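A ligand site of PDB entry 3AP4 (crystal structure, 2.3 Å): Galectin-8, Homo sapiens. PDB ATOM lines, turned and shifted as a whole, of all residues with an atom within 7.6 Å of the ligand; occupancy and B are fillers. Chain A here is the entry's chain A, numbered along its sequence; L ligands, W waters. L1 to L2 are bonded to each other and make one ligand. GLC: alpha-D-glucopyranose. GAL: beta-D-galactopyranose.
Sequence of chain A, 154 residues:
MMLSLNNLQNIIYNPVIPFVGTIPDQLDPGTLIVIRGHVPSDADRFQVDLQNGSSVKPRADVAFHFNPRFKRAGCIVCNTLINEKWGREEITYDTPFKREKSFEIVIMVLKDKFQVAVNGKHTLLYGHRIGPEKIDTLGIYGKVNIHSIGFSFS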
ATOM      1  N   ARG A  45      23.411 -15.744   1.434  1.00  0.00           N
ATOM      2  CA  ARG A  45      24.067 -16.314   2.619  1.00  0.00           C
ATOM      3  C   ARG A  45      25.444 -15.706   2.855  1.00  0.00           C
ATOM      4  O   ARG A  45      26.053 -15.169   1.933  1.00  0.00           O
ATOM      5  CB  ARG A  45      24.240 -17.826   2.485  1.00  0.00           C
ATOM      6  CG  ARG A  45      24.959 -18.260   1.193  1.00  0.00           C
ATOM      7  CD  ARG A  45      25.258 -19.753   1.197  1.00  0.00           C
ATOM      8  NE  ARG A  45      26.424 -20.080   2.022  1.00  0.00           N
ATOM      9  CZ  ARG A  45      26.730 -21.313   2.444  1.00  0.00           C
ATOM     10  NH1 ARG A  45      25.970 -22.346   2.117  1.00  0.00           N
ATOM     11  NH2 ARG A  45      27.811 -21.502   3.198  1.00  0.00           N
ATOM     12  N   PHE A  46      25.922 -15.815   4.083  1.00  0.00           N
ATOM     13  CA  PHE A  46      27.327 -15.563   4.374  1.00  0.00           C
ATOM     14  C   PHE A  46      27.765 -16.531   5.459  1.00  0.00           C
ATOM     15  O   PHE A  46      26.949 -17.293   5.967  1.00  0.00           O
ATOM     16  CB  PHE A  46      27.563 -14.090   4.742  1.00  0.00           C
ATOM     17  CG  PHE A  46      27.125 -13.696   6.130  1.00  0.00           C
ATOM     18  CD1 PHE A  46      25.830 -13.271   6.363  1.00  0.00           C
ATOM     19  CD2 PHE A  46      28.020 -13.691   7.180  1.00  0.00           C
ATOM     20  CE1 PHE A  46      25.413 -12.863   7.640  1.00  0.00           C
ATOM     21  CE2 PHE A  46      27.623 -13.300   8.466  1.00  0.00           C
ATOM     22  CZ  PHE A  46      26.311 -12.887   8.692  1.00  0.00           C
ATOM     23  N   GLN A  47      29.057 -16.526   5.807  1.00  0.00           N
ATOM     24  CA  GLN A  47      29.565 -17.421   6.832  1.00  0.00           C
ATOM     25  C   GLN A  47      30.762 -16.882   7.634  1.00  0.00           C
ATOM     26  O   GLN A  47      31.646 -16.216   7.092  1.00  0.00           O
ATOM     27  CB  GLN A  47      29.900 -18.790   6.209  1.00  0.00           C
ATOM     28  CG  GLN A  47      31.018 -18.760   5.165  1.00  0.00           C
ATOM     29  CD  GLN A  47      31.026 -19.993   4.295  1.00  0.00           C
ATOM     30  OE1 GLN A  47      30.195 -20.144   3.394  1.00  0.00           O
ATOM     31  NE2 GLN A  47      31.967 -20.899   4.558  1.00  0.00           N
ATOM     32  N   ASP A  49      33.651 -18.643   9.774  1.00  0.00           N
ATOM     33  CA  ASP A  49      34.271 -19.964   9.981  1.00  0.00           C
ATOM     34  C   ASP A  49      35.476 -19.876  10.941  1.00  0.00           C
ATOM     35  O   ASP A  49      36.431 -19.146  10.686  1.00  0.00           O
ATOM     36  CB  ASP A  49      34.753 -20.571   8.650  1.00  0.00           C
ATOM     37  CG  ASP A  49      33.610 -20.875   7.679  1.00  0.00           C
ATOM     38  OD1 ASP A  49      32.461 -21.108   8.111  1.00  0.00           O
ATOM     39  OD2 ASP A  49      33.886 -20.900   6.452  1.00  0.00           O
ATOM     40  N   ARG A  59      41.364 -28.330   1.872  1.00  0.00           N
ATOM     41  CA  ARG A  59      40.651 -27.270   2.576  1.00  0.00           C
ATOM     42  C   ARG A  59      40.798 -27.371   4.078  1.00  0.00           C
ATOM     43  O   ARG A  59      40.479 -28.407   4.669  1.00  0.00           O
ATOM     44  CB  ARG A  59      39.165 -27.284   2.202  1.00  0.00           C
ATOM     45  CG  ARG A  59      38.419 -26.087   2.736  1.00  0.00           C
ATOM     46  CD  ARG A  59      36.986 -26.033   2.241  1.00  0.00           C
ATOM     47  NE  ARG A  59      36.205 -25.122   3.072  1.00  0.00           N
ATOM     48  CZ  ARG A  59      34.881 -24.979   3.031  1.00  0.00           C
ATOM     49  NH1 ARG A  59      34.152 -25.682   2.167  1.00  0.00           N
ATOM     50  NH2 ARG A  59      34.284 -24.123   3.853  1.00  0.00           N
ATOM     51  N   HIS A  65      31.430 -23.637  11.762  1.00  0.00           N
ATOM     52  CA  HIS A  65      30.820 -23.001  10.605  1.00  0.00           C
ATOM     53  C   HIS A  65      29.504 -22.393  11.051  1.00  0.00           C
ATOM     54  O   HIS A  65      28.594 -23.122  11.433  1.00  0.00           O
ATOM     55  CB  HIS A  65      30.586 -24.057   9.533  1.00  0.00           C
ATOM     56  CG  HIS A  65      29.934 -23.552   8.276  1.00  0.00           C
ATOM     57  ND1 HIS A  65      30.495 -22.578   7.483  1.00  0.00           N
ATOM     58  CD2 HIS A  65      28.806 -23.953   7.639  1.00  0.00           C
ATOM     59  CE1 HIS A  65      29.730 -22.372   6.427  1.00  0.00           C
ATOM     60  NE2 HIS A  65      28.696 -23.192   6.500  1.00  0.00           N
ATOM     61  N   PHE A  66      29.426 -21.061  11.057  1.00  0.00           N
ATOM     62  CA  PHE A  66      28.222 -20.308  11.426  1.00  0.00           C
ATOM     63  C   PHE A  66      27.743 -19.596  10.169  1.00  0.00           C
ATOM     64  O   PHE A  66      28.353 -18.616   9.732  1.00  0.00           O
ATOM     65  CB  PHE A  66      28.572 -19.311  12.526  1.00  0.00           C
ATOM     66  CG  PHE A  66      27.426 -18.465  12.992  1.00  0.00           C
ATOM     67  CD1 PHE A  66      26.637 -18.867  14.052  1.00  0.00           C
ATOM     68  CD2 PHE A  66      27.190 -17.225  12.426  1.00  0.00           C
ATOM     69  CE1 PHE A  66      25.585 -18.074  14.516  1.00  0.00           C
ATOM     70  CE2 PHE A  66      26.142 -16.422  12.880  1.00  0.00           C
ATOM     71  CZ  PHE A  66      25.337 -16.856  13.935  1.00  0.00           C
ATOM     72  N   ASN A  67      26.635 -20.101   9.619  1.00  0.00           N
ATOM     73  CA  ASN A  67      26.235 -19.824   8.234  1.00  0.00           C
ATOM     74  C   ASN A  67      24.781 -19.353   8.151  1.00  0.00           C
ATOM     75  O   ASN A  67      23.895 -20.158   7.939  1.00  0.00           O
ATOM     76  CB  ASN A  67      26.448 -21.106   7.407  1.00  0.00           C
ATOM     77  CG  ASN A  67      25.976 -21.000   5.954  1.00  0.00           C
ATOM     78  OD1 ASN A  67      25.518 -21.993   5.383  1.00  0.00           O
ATOM     79  ND2 ASN A  67      26.101 -19.812   5.344  1.00  0.00           N
ATOM     80  N   ARG A  69      21.466 -18.001   6.476  1.00  0.00           N
ATOM     81  CA  ARG A  69      20.881 -18.209   5.148  1.00  0.00           C
ATOM     82  C   ARG A  69      19.555 -17.486   5.056  1.00  0.00           C
ATOM     83  O   ARG A  69      18.747 -17.587   5.971  1.00  0.00           O
ATOM     84  CB  ARG A  69      20.690 -19.702   4.863  1.00  0.00           C
ATOM     85  CG  ARG A  69      21.952 -20.409   4.365  1.00  0.00           C
ATOM     86  CD  ARG A  69      21.775 -21.917   4.314  1.00  0.00           C
ATOM     87  NE  ARG A  69      23.044 -22.638   4.360  1.00  0.00           N
ATOM     88  CZ  ARG A  69      23.188 -23.937   4.133  1.00  0.00           C
ATOM     89  NH1 ARG A  69      22.136 -24.683   3.829  1.00  0.00           N
ATOM     90  NH2 ARG A  69      24.395 -24.503   4.181  1.00  0.00           N
ATOM     91  N   LYS A  71      17.151 -17.346   2.233  1.00  0.00           N
ATOM     92  CA  LYS A  71      16.060 -17.809   1.364  1.00  0.00           C
ATOM     93  C   LYS A  71      14.799 -18.046   2.204  1.00  0.00           C
ATOM     94  O   LYS A  71      14.877 -18.529   3.343  1.00  0.00           O
ATOM     95  CB  LYS A  71      16.458 -19.074   0.558  1.00  0.00           C
ATOM     96  CG  LYS A  71      15.809 -20.385   1.075  1.00  0.00           C
ATOM     97  CD  LYS A  71      16.314 -21.672   0.412  1.00  0.00           C
ATOM     98  CE  LYS A  71      15.490 -22.877   0.929  1.00  0.00           C
ATOM     99  NZ  LYS A  71      16.001 -24.210   0.475  1.00  0.00           N
ATOM    100  N   VAL A  77      22.649 -22.131   9.755  1.00  0.00           N
ATOM    101  CA  VAL A  77      23.167 -23.486   9.716  1.00  0.00           C
ATOM    102  C   VAL A  77      24.550 -23.523  10.384  1.00  0.00           C
ATOM    103  O   VAL A  77      25.429 -22.725  10.031  1.00  0.00           O
ATOM    104  CB  VAL A  77      23.256 -23.994   8.285  1.00  0.00           C
ATOM    105  CG1 VAL A  77      24.038 -25.309   8.201  1.00  0.00           C
ATOM    106  CG2 VAL A  77      21.839 -24.134   7.726  1.00  0.00           C
ATOM    107  N   CYS A  78      24.711 -24.412  11.353  1.00  0.00           N
ATOM    108  CA  CYS A  78      26.023 -24.640  11.954  1.00  0.00           C
ATOM    109  C   CYS A  78      26.498 -26.064  11.693  1.00  0.00           C
ATOM    110  O   CYS A  78      25.708 -27.001  11.655  1.00  0.00           O
ATOM    111  CB  CYS A  78      26.014 -24.322  13.456  1.00  0.00           C
ATOM    112  SG  CYS A  78      25.510 -22.629  13.870  1.00  0.00           S
ATOM    113  N   ASN A  79      27.810 -26.213  11.503  1.00  0.00           N
ATOM    114  CA  ASN A  79      28.404 -27.500  11.179  1.00  0.00           C
ATOM    115  C   ASN A  79      29.902 -27.424  11.426  1.00  0.00           C
ATOM    116  O   ASN A  79      30.403 -26.393  11.906  1.00  0.00           O
ATOM    117  CB  ASN A  79      28.125 -27.842   9.699  1.00  0.00           C
ATOM    118  CG  ASN A  79      27.995 -29.360   9.430  1.00  0.00           C
ATOM    119  OD1 ASN A  79      27.492 -29.753   8.379  1.00  0.00           O
ATOM    120  ND2 ASN A  79      28.440 -30.186  10.352  1.00  0.00           N
ATOM    121  N   THR A  80      30.595 -28.519  11.126  1.00  0.00           N
ATOM    122  CA  THR A  80      32.033 -28.619  11.224  1.00  0.00           C
ATOM    123  C   THR A  80      32.549 -29.289   9.963  1.00  0.00           C
ATOM    124  O   THR A  80      31.921 -30.221   9.472  1.00  0.00           O
ATOM    125  CB  THR A  80      32.402 -29.453  12.439  1.00  0.00           C
ATOM    126  OG1 THR A  80      32.064 -28.722  13.621  1.00  0.00           O
ATOM    127  CG2 THR A  80      33.918 -29.813  12.447  1.00  0.00           C
ATOM    128  N   LEU A  81      33.665 -28.803   9.435  1.00  0.00           N
ATOM    129  CA  LEU A  81      34.332 -29.414   8.267  1.00  0.00           C
ATOM    130  C   LEU A  81      35.619 -30.116   8.742  1.00  0.00           C
ATOM    131  O   LEU A  81      36.556 -29.460   9.218  1.00  0.00           O
ATOM    132  CB  LEU A  81      34.659 -28.369   7.203  1.00  0.00           C
ATOM    133  CG  LEU A  81      35.213 -28.880   5.856  1.00  0.00           C
ATOM    134  CD1 LEU A  81      34.101 -29.417   4.980  1.00  0.00           C
ATOM    135  CD2 LEU A  81      36.007 -27.804   5.102  1.00  0.00           C
ATOM    136  N   TRP A  86      31.622 -32.340   5.428  1.00  0.00           N
ATOM    137  CA  TRP A  86      30.717 -31.742   6.412  1.00  0.00           C
ATOM    138  C   TRP A  86      30.071 -32.808   7.280  1.00  0.00           C
ATOM    139  O   TRP A  86      29.775 -33.892   6.789  1.00  0.00           O
ATOM    140  CB  TRP A  86      29.634 -30.908   5.693  1.00  0.00           C
ATOM    141  CG  TRP A  86      30.190 -29.662   5.074  1.00  0.00           C
ATOM    142  CD1 TRP A  86      30.389 -29.429   3.754  1.00  0.00           C
ATOM    143  CD2 TRP A  86      30.639 -28.501   5.778  1.00  0.00           C
ATOM    144  NE1 TRP A  86      30.947 -28.174   3.579  1.00  0.00           N
ATOM    145  CE2 TRP A  86      31.097 -27.588   4.804  1.00  0.00           C
ATOM    146  CE3 TRP A  86      30.690 -28.127   7.118  1.00  0.00           C
ATOM    147  CZ2 TRP A  86      31.608 -26.325   5.140  1.00  0.00           C
ATOM    148  CZ3 TRP A  86      31.194 -26.885   7.452  1.00  0.00           C
ATOM    149  CH2 TRP A  86      31.647 -25.994   6.467  1.00  0.00           C
ATOM    150  N   GLY A  87      29.841 -32.494   8.551  1.00  0.00           N
ATOM    151  CA  GLY A  87      29.173 -33.398   9.481  1.00  0.00           C
ATOM    152  C   GLY A  87      27.691 -33.107   9.597  1.00  0.00           C
ATOM    153  O   GLY A  87      27.085 -32.555   8.693  1.00  0.00           O
ATOM    154  N   ARG A  88      27.108 -33.497  10.732  1.00  0.00           N
ATOM    155  CA  ARG A  88      25.695 -33.230  11.007  1.00  0.00           C
ATOM    156  C   ARG A  88      25.453 -31.715  11.123  1.00  0.00           C
ATOM    157  O   ARG A  88      26.187 -31.022  11.817  1.00  0.00           O
ATOM    158  CB  ARG A  88      25.248 -33.909  12.314  1.00  0.00           C
ATOM    159  CG  ARG A  88      24.474 -35.204  12.151  1.00  0.00           C
ATOM    160  CD  ARG A  88      25.378 -36.450  12.041  1.00  0.00           C
ATOM    161  NE  ARG A  88      26.046 -36.536  10.750  1.00  0.00           N
ATOM    162  CZ  ARG A  88      26.706 -37.605  10.284  1.00  0.00           C
ATOM    163  NH1 ARG A  88      26.777 -38.729  11.006  1.00  0.00           N
ATOM    164  NH2 ARG A  88      27.275 -37.552   9.089  1.00  0.00           N
ATOM    165  N   GLU A  89      24.422 -31.227  10.425  1.00  0.00           N
ATOM    166  CA  GLU A  89      24.023 -29.820  10.479  1.00  0.00           C
ATOM    167  C   GLU A  89      23.175 -29.572  11.713  1.00  0.00           C
ATOM    168  O   GLU A  89      22.348 -30.407  12.056  1.00  0.00           O
ATOM    169  CB  GLU A  89      23.235 -29.418   9.212  1.00  0.00           C
ATOM    170  CG  GLU A  89      24.069 -29.378   7.931  1.00  0.00           C
ATOM    171  CD  GLU A  89      23.290 -28.871   6.719  1.00  0.00           C
ATOM    172  OE1 GLU A  89      22.044 -28.950   6.706  1.00  0.00           O
ATOM    173  OE2 GLU A  89      23.932 -28.394   5.759  1.00  0.00           O
ATOM    174  N   GLU A  90      23.384 -28.435  12.372  1.00  0.00           N
ATOM    175  CA  GLU A  90      22.493 -27.980  13.442  1.00  0.00           C
ATOM    176  C   GLU A  90      21.853 -26.669  12.967  1.00  0.00           C
ATOM    177  O   GLU A  90      22.532 -25.643  12.827  1.00  0.00           O
ATOM    178  CB  GLU A  90      23.240 -27.818  14.783  1.00  0.00           C
ATOM    179  CG  GLU A  90      24.046 -29.079  15.184  1.00  0.00           C
ATOM    180  CD  GLU A  90      24.809 -28.967  16.502  1.00  0.00           C
ATOM    181  OE1 GLU A  90      24.457 -28.137  17.371  1.00  0.00           O
ATOM    182  OE2 GLU A  90      25.769 -29.747  16.682  1.00  0.00           O
ATOM    183  N   ILE A  91      20.562 -26.720  12.685  1.00  0.00           N
ATOM    184  CA  ILE A  91      19.861 -25.614  12.072  1.00  0.00           C
ATOM    185  C   ILE A  91      19.045 -24.883  13.121  1.00  0.00           C
ATOM    186  O   ILE A  91      18.201 -25.486  13.786  1.00  0.00           O
ATOM    187  CB  ILE A  91      18.922 -26.091  10.941  1.00  0.00           C
ATOM    188  CG1 ILE A  91      19.700 -26.963   9.946  1.00  0.00           C
ATOM    189  CG2 ILE A  91      18.326 -24.893  10.206  1.00  0.00           C
ATOM    190  CD1 ILE A  91      18.835 -27.631   8.873  1.00  0.00           C
HETATM  191  C1  GLC L   1      22.493 -30.610   1.767  1.00  0.00           C
HETATM  192  C2  GLC L   1      22.249 -29.411   2.746  1.00  0.00           C
HETATM  193  C3  GLC L   1      23.019 -28.146   2.291  1.00  0.00           C
HETATM  194  C4  GLC L   1      24.507 -28.521   2.104  1.00  0.00           C
HETATM  195  C5  GLC L   1      24.559 -29.548   0.933  1.00  0.00           C
HETATM  196  C6  GLC L   1      26.003 -30.052   0.677  1.00  0.00           C
HETATM  197  O1  GLC L   1      21.612 -30.696   0.703  1.00  0.00           O
HETATM  198  O2  GLC L   1      20.889 -29.041   2.835  1.00  0.00           O
HETATM  199  O3  GLC L   1      22.969 -27.188   3.314  1.00  0.00           O
HETATM  200  O4  GLC L   1      25.220 -27.323   1.779  1.00  0.00           O
HETATM  201  O5  GLC L   1      23.801 -30.722   1.228  1.00  0.00           O
HETATM  202  O6  GLC L   1      26.595 -30.590   1.823  1.00  0.00           O
HETATM  203  C1  GAL L   2      26.505 -27.133   2.357  1.00  0.00           C
HETATM  204  C2  GAL L   2      27.118 -25.855   1.696  1.00  0.00           C
HETATM  205  C3  GAL L   2      28.399 -25.469   2.494  1.00  0.00           C
HETATM  206  C4  GAL L   2      28.105 -25.386   4.015  1.00  0.00           C
HETATM  207  C5  GAL L   2      27.401 -26.685   4.477  1.00  0.00           C
HETATM  208  C6  GAL L   2      27.029 -26.610   5.977  1.00  0.00           C
HETATM  209  O2  GAL L   2      27.522 -26.136   0.389  1.00  0.00           O
HETATM  210  O3  GAL L   2      28.931 -24.200   2.114  1.00  0.00           O
HETATM  211  O4  GAL L   2      27.291 -24.298   4.373  1.00  0.00           O
HETATM  212  O5  GAL L   2      26.215 -26.928   3.725  1.00  0.00           O
HETATM  213  O6  GAL L   2      26.443 -27.777   6.462  1.00  0.00           O
HETATM  214  O   HOH W   1      26.186 -30.577   4.576  1.00  0.00           O
HETATM  215  O   HOH W   2      25.214 -25.943  -1.434  1.00  0.00           O
HETATM  216  O   HOH W   3      20.191 -27.905   5.155  1.00  0.00           O
HETATM  217  O   HOH W   4      31.695 -23.425   2.896  1.00  0.00           O
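Water W3 bridges OE1 of Glu 89 (2.6 Å) and O2 of GLC L1 (2.7 Å).
Water W1 bridges O6 of GLC L1 (2.8 Å) and OE2 of Glu 89 (3.4 Å).
Water W4 lies within hydrogen-bond range of the guanidinium group of Arg 59, an oxygen (O3) of GAL L2 and the side-chain amide nitrogen of Gln 47.
Val 77 touches the ligand.
Trp 86 touches the ligand.
Hydrophobic or aromatic side chains within 4 Å of the ligand: His 65, Val 77 and Trp 86.
Of the 21 residues printed, 8 come within 4 Å of the ligand.
Along chain A the residues within 4 Å of the ligand span positions 45 to 89.
OD1 of Asn 79 lies within hydrogen-bond range of O6 of GAL L2, at 2.9 Å.
The side-chain carboxylate (OE2) of Glu 89 is in hydrogen-bond range of an oxygen (O6) of GAL L2 (2.7 Å).
An oxygen (O4) of GAL L2 lies within hydrogen-bond range of the guanidinium group of Arg 45, 3.1 Å away.
A ring nitrogen (NE2) of His 65 is in hydrogen-bond range of an oxygen (O4) of GAL L2, at 2.8 Å.
The guanidinium group (NH1) of Arg 69 lies within hydrogen-bond range of an oxygen (O3) of GLC L1 (2.7 Å).
OD1 of Asn 67 is in hydrogen-bond range of O4 of GAL L2.
The backbone carbonyl oxygen (O) of Val 77 is in hydrogen-bond range of the backbone NH (N) of Asn 67, at 2.9 Å.
The backbone NH of His 65 lies within hydrogen-bond range of the backbone carbonyl oxygen of Asn 79.
NE of Arg 69 sits at hydrogen-bond distance from OD1 of Asn 67 (2.8 Å).
The guanidinium group (NH2) of Arg 45 is in hydrogen-bond range of the side-chain amide oxygen (OE1) of Gln 47 (2.8 Å).
The side-chain amide nitrogen of Asn 79 lies within hydrogen-bond range of the backbone carbonyl oxygen of Arg 88 (2.8 Å).
ND2 of Asn 67 is in hydrogen-bond range of O of Phe 46.
A ring nitrogen (ND1) of His 65 lies within hydrogen-bond range of the side-chain carboxylate of Asp 49 (2.5 Å).
O of Gly 87 sits close to OD1 of Asn 79 (2.8 Å).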
